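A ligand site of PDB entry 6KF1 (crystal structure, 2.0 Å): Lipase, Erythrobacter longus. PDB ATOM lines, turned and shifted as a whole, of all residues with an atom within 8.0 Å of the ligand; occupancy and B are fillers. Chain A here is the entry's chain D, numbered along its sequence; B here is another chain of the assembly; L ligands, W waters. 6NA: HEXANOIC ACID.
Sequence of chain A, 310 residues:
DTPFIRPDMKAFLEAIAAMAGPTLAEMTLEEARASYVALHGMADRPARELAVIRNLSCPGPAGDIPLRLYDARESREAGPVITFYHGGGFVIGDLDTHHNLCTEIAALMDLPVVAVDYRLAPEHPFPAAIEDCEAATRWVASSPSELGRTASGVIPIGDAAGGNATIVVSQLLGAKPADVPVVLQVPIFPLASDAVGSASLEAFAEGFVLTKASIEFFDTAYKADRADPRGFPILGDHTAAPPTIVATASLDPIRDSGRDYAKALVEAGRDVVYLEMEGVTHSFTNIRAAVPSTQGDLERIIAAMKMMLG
NH1 of Arg 259 lies within salt-bridge range of O of the ligand (2.9 Å).
O of the ligand is in salt-bridge range of NH2 of Arg 255 (3.6 Å).
NH1 of Arg 259 lies within hydrogen-bond range of O of Glu 266 of chain B (3.1 Å).
The side-chain carboxylate (OD1) of Asp 256 lies within salt-bridge range of the guanidinium group (NH1) of Arg 259 (3.9 Å).
The guanidinium group (NH2) of Arg 259 is in salt-bridge range of the side-chain carboxylate (OE2) of Glu 276, 2.8 Å away.
The side-chain carboxylate of Asp 256 is in salt-bridge range of the guanidinium group of Arg 255, at 3.0 Å.
NH1 of Arg 255 sits at hydrogen-bond distance from O of Ser 250 (3.1 Å).
Ala 199 touches the ligand (O to C6, 3.6 Å).
Ala 203 touches the ligand (CB to C6, 3.97 Å).
CZ of Phe 204 touches CG of the ligand, at 3.9 Å.
Hydrophobic or aromatic side chains that line the ligand: Ala 199, Ala 203 and Phe 204.
Of the 23 residues printed, 5 come within 4 Å of the ligand.
Water W1 bridges O of the ligand (2.9 Å) and O of Glu 266 of chain B (2.9 Å).
Water W3 lies within hydrogen-bond range of O of Ala 267 of chain B (2.8 Å) and OXT of the ligand (3.1 Å).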
ATOM      1  N   ASP A   1      15.922 -12.891  15.360  1.00  0.00           N
ATOM      2  CA  ASP A   1      14.462 -12.894  15.551  1.00  0.00           C
ATOM      3  C   ASP A   1      13.798 -12.361  14.264  1.00  0.00           C
ATOM      4  O   ASP A   1      14.472 -12.332  13.218  1.00  0.00           O
ATOM      5  CB  ASP A   1      14.097 -12.090  16.803  1.00  0.00           C
ATOM      6  CG  ASP A   1      12.752 -12.465  17.415  1.00  0.00           C
ATOM      7  OD1 ASP A   1      12.437 -13.683  17.455  1.00  0.00           O
ATOM      8  OD2 ASP A   1      12.035 -11.552  17.831  1.00  0.00           O
ATOM      9  N   PRO A   3      11.826  -8.943  14.287  1.00  0.00           N
ATOM     10  CA  PRO A   3      11.335  -7.815  15.095  1.00  0.00           C
ATOM     11  C   PRO A   3      10.161  -7.193  14.361  1.00  0.00           C
ATOM     12  O   PRO A   3      10.020  -7.373  13.159  1.00  0.00           O
ATOM     13  CB  PRO A   3      12.546  -6.875  15.199  1.00  0.00           C
ATOM     14  CG  PRO A   3      13.297  -7.177  13.906  1.00  0.00           C
ATOM     15  CD  PRO A   3      13.170  -8.683  13.744  1.00  0.00           C
ATOM     16  N   SER A 198      26.752  -3.616  22.191  1.00  0.00           N
ATOM     17  CA  SER A 198      25.319  -3.579  22.585  1.00  0.00           C
ATOM     18  C   SER A 198      24.549  -4.675  21.877  1.00  0.00           C
ATOM     19  O   SER A 198      24.863  -5.021  20.725  1.00  0.00           O
ATOM     20  CB  SER A 198      24.717  -2.200  22.358  1.00  0.00           C
ATOM     21  OG  SER A 198      24.591  -1.844  20.976  1.00  0.00           O
ATOM     22  N   ALA A 199      23.491  -5.153  22.507  1.00  0.00           N
ATOM     23  CA  ALA A 199      22.569  -6.134  21.929  1.00  0.00           C
ATOM     24  C   ALA A 199      21.855  -5.501  20.718  1.00  0.00           C
ATOM     25  O   ALA A 199      21.660  -6.185  19.676  1.00  0.00           O
ATOM     26  CB  ALA A 199      21.614  -6.613  22.997  1.00  0.00           C
ATOM     27  N   SER A 200      21.468  -4.223  20.792  1.00  0.00           N
ATOM     28  CA  SER A 200      20.763  -3.611  19.634  1.00  0.00           C
ATOM     29  C   SER A 200      21.716  -3.561  18.409  1.00  0.00           C
ATOM     30  O   SER A 200      21.206  -3.744  17.281  1.00  0.00           O
ATOM     31  CB  SER A 200      20.123  -2.264  19.954  1.00  0.00           C
ATOM     32  OG  SER A 200      21.072  -1.346  20.473  1.00  0.00           O
ATOM     33  N   LEU A 201      22.990  -3.260  18.572  1.00  0.00           N
ATOM     34  CA  LEU A 201      23.911  -3.156  17.409  1.00  0.00           C
ATOM     35  C   LEU A 201      23.965  -4.512  16.688  1.00  0.00           C
ATOM     36  O   LEU A 201      23.804  -4.511  15.462  1.00  0.00           O
ATOM     37  CB  LEU A 201      25.287  -2.687  17.859  1.00  0.00           C
ATOM     38  CG  LEU A 201      26.360  -2.615  16.765  1.00  0.00           C
ATOM     39  CD1 LEU A 201      25.977  -1.668  15.635  1.00  0.00           C
ATOM     40  CD2 LEU A 201      27.682  -2.223  17.369  1.00  0.00           C
ATOM     41  N   GLU A 202      24.014  -5.622  17.445  1.00  0.00           N
ATOM     42  CA  GLU A 202      24.089  -6.992  16.893  1.00  0.00           C
ATOM     43  C   GLU A 202      22.772  -7.274  16.175  1.00  0.00           C
ATOM     44  O   GLU A 202      22.825  -7.727  15.052  1.00  0.00           O
ATOM     45  CB  GLU A 202      24.382  -8.028  17.973  1.00  0.00           C
ATOM     46  N   ALA A 203      21.620  -6.960  16.764  1.00  0.00           N
ATOM     47  CA  ALA A 203      20.310  -7.318  16.173  1.00  0.00           C
ATOM     48  C   ALA A 203      20.089  -6.527  14.870  1.00  0.00           C
ATOM     49  O   ALA A 203      19.358  -7.028  14.019  1.00  0.00           O
ATOM     50  CB  ALA A 203      19.189  -7.097  17.166  1.00  0.00           C
ATOM     51  N   PHE A 204      20.512  -5.270  14.810  1.00  0.00           N
ATOM     52  CA  PHE A 204      20.087  -4.310  13.742  1.00  0.00           C
ATOM     53  C   PHE A 204      21.294  -3.841  12.915  1.00  0.00           C
ATOM     54  O   PHE A 204      21.221  -2.753  12.314  1.00  0.00           O
ATOM     55  CB  PHE A 204      19.281  -3.143  14.353  1.00  0.00           C
ATOM     56  CG  PHE A 204      18.147  -3.618  15.225  1.00  0.00           C
ATOM     57  CD1 PHE A 204      17.179  -4.467  14.717  1.00  0.00           C
ATOM     58  CD2 PHE A 204      18.047  -3.219  16.551  1.00  0.00           C
ATOM     59  CE1 PHE A 204      16.165  -4.966  15.528  1.00  0.00           C
ATOM     60  CE2 PHE A 204      17.025  -3.713  17.365  1.00  0.00           C
ATOM     61  CZ  PHE A 204      16.095  -4.602  16.857  1.00  0.00           C
ATOM     62  N   SER A 250      12.769   1.426  17.957  1.00  0.00           N
ATOM     63  CA  SER A 250      12.825  -0.007  18.398  1.00  0.00           C
ATOM     64  C   SER A 250      13.790  -0.826  17.522  1.00  0.00           C
ATOM     65  O   SER A 250      14.301  -1.812  18.029  1.00  0.00           O
ATOM     66  CB  SER A 250      11.473  -0.641  18.440  1.00  0.00           C
ATOM     67  OG  SER A 250      10.825  -0.725  17.185  1.00  0.00           O
ATOM     68  N   LEU A 251      14.033  -0.421  16.258  1.00  0.00           N
ATOM     69  CA  LEU A 251      14.926  -1.157  15.294  1.00  0.00           C
ATOM     70  C   LEU A 251      16.259  -0.443  15.153  1.00  0.00           C
ATOM     71  O   LEU A 251      16.962  -0.736  14.198  1.00  0.00           O
ATOM     72  CB  LEU A 251      14.233  -1.201  13.923  1.00  0.00           C
ATOM     73  CG  LEU A 251      12.834  -1.790  13.936  1.00  0.00           C
ATOM     74  CD1 LEU A 251      12.118  -1.574  12.610  1.00  0.00           C
ATOM     75  CD2 LEU A 251      12.904  -3.253  14.298  1.00  0.00           C
ATOM     76  N   ASP A 252      16.587   0.524  16.015  1.00  0.00           N
ATOM     77  CA  ASP A 252      17.861   1.269  15.895  1.00  0.00           C
ATOM     78  C   ASP A 252      19.015   0.452  16.441  1.00  0.00           C
ATOM     79  O   ASP A 252      18.991  -0.014  17.583  1.00  0.00           O
ATOM     80  CB  ASP A 252      17.753   2.631  16.595  1.00  0.00           C
ATOM     81  CG  ASP A 252      18.823   3.605  16.242  1.00  0.00           C
ATOM     82  OD1 ASP A 252      19.907   3.141  15.810  1.00  0.00           O
ATOM     83  OD2 ASP A 252      18.589   4.827  16.453  1.00  0.00           O
ATOM     84  N   ARG A 255      19.728   2.013  19.613  1.00  0.00           N
ATOM     85  CA  ARG A 255      18.565   2.057  20.557  1.00  0.00           C
ATOM     86  C   ARG A 255      19.054   1.893  21.999  1.00  0.00           C
ATOM     87  O   ARG A 255      18.621   2.687  22.864  1.00  0.00           O
ATOM     88  CB  ARG A 255      17.603   0.926  20.245  1.00  0.00           C
ATOM     89  CG  ARG A 255      16.370   0.873  21.143  1.00  0.00           C
ATOM     90  CD  ARG A 255      15.731  -0.466  20.967  1.00  0.00           C
ATOM     91  NE  ARG A 255      16.562  -1.494  21.558  1.00  0.00           N
ATOM     92  CZ  ARG A 255      16.300  -2.800  21.420  1.00  0.00           C
ATOM     93  NH1 ARG A 255      15.289  -3.154  20.664  1.00  0.00           N
ATOM     94  NH2 ARG A 255      17.061  -3.709  22.006  1.00  0.00           N
ATOM     95  N   ASP A 256      19.878   0.867  22.252  1.00  0.00           N
ATOM     96  CA  ASP A 256      20.313   0.543  23.648  1.00  0.00           C
ATOM     97  C   ASP A 256      21.122   1.686  24.268  1.00  0.00           C
ATOM     98  O   ASP A 256      21.094   1.805  25.518  1.00  0.00           O
ATOM     99  CB  ASP A 256      21.085  -0.765  23.749  1.00  0.00           C
ATOM    100  CG  ASP A 256      20.202  -1.960  23.486  1.00  0.00           C
ATOM    101  OD1 ASP A 256      18.995  -1.764  23.235  1.00  0.00           O
ATOM    102  OD2 ASP A 256      20.751  -3.120  23.547  1.00  0.00           O
ATOM    103  N   ARG A 259      18.456   3.987  25.628  1.00  0.00           N
ATOM    104  CA  ARG A 259      17.969   3.327  26.864  1.00  0.00           C
ATOM    105  C   ARG A 259      18.949   3.606  27.994  1.00  0.00           C
ATOM    106  O   ARG A 259      18.522   4.018  29.132  1.00  0.00           O
ATOM    107  CB  ARG A 259      17.786   1.827  26.638  1.00  0.00           C
ATOM    108  CG  ARG A 259      16.572   1.427  25.822  1.00  0.00           C
ATOM    109  CD  ARG A 259      16.504  -0.105  25.692  1.00  0.00           C
ATOM    110  NE  ARG A 259      15.420  -0.464  24.782  1.00  0.00           N
ATOM    111  CZ  ARG A 259      15.088  -1.722  24.483  1.00  0.00           C
ATOM    112  NH1 ARG A 259      15.726  -2.711  25.044  1.00  0.00           N
ATOM    113  NH2 ARG A 259      14.119  -1.992  23.655  1.00  0.00           N
ATOM    114  N   GLU A 276      10.033   5.180  23.010  1.00  0.00           N
ATOM    115  CA  GLU A 276      10.714   4.220  22.088  1.00  0.00           C
ATOM    116  C   GLU A 276       9.703   3.907  20.987  1.00  0.00           C
ATOM    117  O   GLU A 276       8.671   3.234  21.234  1.00  0.00           O
ATOM    118  CB  GLU A 276      11.269   3.037  22.863  1.00  0.00           C
ATOM    119  CG  GLU A 276      11.896   1.983  21.965  1.00  0.00           C
ATOM    120  CD  GLU A 276      12.680   0.905  22.660  1.00  0.00           C
ATOM    121  OE1 GLU A 276      13.454   1.247  23.565  1.00  0.00           O
ATOM    122  OE2 GLU A 276      12.487  -0.241  22.253  1.00  0.00           O
ATOM    123  N   GLU A 278       7.824   2.368  18.050  1.00  0.00           N
ATOM    124  CA  GLU A 278       7.614   0.920  17.774  1.00  0.00           C
ATOM    125  C   GLU A 278       7.563   0.670  16.245  1.00  0.00           C
ATOM    126  O   GLU A 278       6.698   1.232  15.559  1.00  0.00           O
ATOM    127  CB  GLU A 278       6.353   0.392  18.445  1.00  0.00           C
ATOM    128  CG  GLU A 278       6.494   0.248  19.949  1.00  0.00           C
ATOM    129  CD  GLU A 278       7.601  -0.722  20.335  1.00  0.00           C
ATOM    130  OE1 GLU A 278       8.285  -0.482  21.336  1.00  0.00           O
ATOM    131  OE2 GLU A 278       7.812  -1.702  19.589  1.00  0.00           O
ATOM    132  N   THR B 238       8.123  -6.493  29.726  1.00  0.00           N
ATOM    133  CA  THR B 238       8.267  -6.415  28.248  1.00  0.00           C
ATOM    134  C   THR B 238       7.036  -5.882  27.550  1.00  0.00           C
ATOM    135  O   THR B 238       7.185  -5.378  26.371  1.00  0.00           O
ATOM    136  CB  THR B 238       8.728  -7.746  27.620  1.00  0.00           C
ATOM    137  OG1 THR B 238       7.767  -8.755  27.897  1.00  0.00           O
ATOM    138  CG2 THR B 238      10.082  -8.142  28.160  1.00  0.00           C
ATOM    139  N   VAL B 265      12.448   1.407  31.028  1.00  0.00           N
ATOM    140  CA  VAL B 265      13.321   1.883  29.908  1.00  0.00           C
ATOM    141  C   VAL B 265      14.152   0.690  29.398  1.00  0.00           C
ATOM    142  O   VAL B 265      14.276   0.513  28.167  1.00  0.00           O
ATOM    143  CB  VAL B 265      14.237   3.024  30.338  1.00  0.00           C
ATOM    144  CG1 VAL B 265      15.254   3.369  29.247  1.00  0.00           C
ATOM    145  CG2 VAL B 265      13.478   4.241  30.846  1.00  0.00           C
ATOM    146  N   GLU B 266      14.674  -0.119  30.319  1.00  0.00           N
ATOM    147  CA  GLU B 266      15.464  -1.324  30.004  1.00  0.00           C
ATOM    148  C   GLU B 266      14.659  -2.207  29.056  1.00  0.00           C
ATOM    149  O   GLU B 266      15.280  -2.798  28.117  1.00  0.00           O
ATOM    150  CB  GLU B 266      15.953  -2.051  31.260  1.00  0.00           C
ATOM    151  CG  GLU B 266      16.694  -3.387  30.971  1.00  0.00           C
ATOM    152  CD  GLU B 266      18.004  -3.244  30.214  1.00  0.00           C
ATOM    153  OE1 GLU B 266      18.622  -2.172  30.300  1.00  0.00           O
ATOM    154  OE2 GLU B 266      18.385  -4.196  29.500  1.00  0.00           O
ATOM    155  N   ALA B 267      13.330  -2.298  29.210  1.00  0.00           N
ATOM    156  CA  ALA B 267      12.471  -3.198  28.430  1.00  0.00           C
ATOM    157  C   ALA B 267      11.913  -2.458  27.193  1.00  0.00           C
ATOM    158  O   ALA B 267      11.035  -2.993  26.510  1.00  0.00           O
ATOM    159  CB  ALA B 267      11.387  -3.777  29.325  1.00  0.00           C
ATOM    160  N   GLY B 268      12.346  -1.222  26.967  1.00  0.00           N
ATOM    161  CA  GLY B 268      11.904  -0.444  25.795  1.00  0.00           C
ATOM    162  C   GLY B 268      10.504   0.107  25.927  1.00  0.00           C
ATOM    163  O   GLY B 268       9.842   0.355  24.892  1.00  0.00           O
ATOM    164  N   ARG B 269      10.026   0.372  27.138  1.00  0.00           N
ATOM    165  CA  ARG B 269       8.618   0.799  27.299  1.00  0.00           C
ATOM    166  C   ARG B 269       8.577   2.323  27.434  1.00  0.00           C
ATOM    167  O   ARG B 269       9.508   2.868  27.928  1.00  0.00           O
ATOM    168  CB  ARG B 269       7.969   0.128  28.531  1.00  0.00           C
ATOM    169  CG  ARG B 269       8.189  -1.378  28.590  1.00  0.00           C
ATOM    170  CD  ARG B 269       7.800  -2.098  27.307  1.00  0.00           C
ATOM    171  NE  ARG B 269       6.395  -1.975  27.020  1.00  0.00           N
ATOM    172  CZ  ARG B 269       5.850  -1.988  25.810  1.00  0.00           C
ATOM    173  NH1 ARG B 269       6.617  -2.120  24.732  1.00  0.00           N
ATOM    174  NH2 ARG B 269       4.554  -1.863  25.683  1.00  0.00           N
HETATM  175  CA  6NA L   1      14.701  -6.862  22.633  1.00  0.00           C
HETATM  176  C   6NA L   1      14.407  -5.778  23.645  1.00  0.00           C
HETATM  177  O   6NA L   1      15.300  -5.559  24.534  1.00  0.00           O
HETATM  178  CB  6NA L   1      14.550  -6.483  21.183  1.00  0.00           C
HETATM  179  CG  6NA L   1      15.863  -6.316  20.400  1.00  0.00           C
HETATM  180  CD  6NA L   1      17.013  -7.295  20.626  1.00  0.00           C
HETATM  181  C6  6NA L   1      18.301  -6.675  21.009  1.00  0.00           C
HETATM  182  OXT 6NA L   1      13.334  -5.097  23.508  1.00  0.00           O
HETATM  183  O   HOH W   1      15.662  -5.599  27.400  1.00  0.00           O
HETATM  184  O   HOH W   2      13.628  -6.773  18.568  1.00  0.00           O
HETATM  185  O   HOH W   3      11.570  -5.667  26.052  1.00  0.00           O
HETATM  186  O   HOH W   4      12.271  -8.203  21.704  1.00  0.00           O
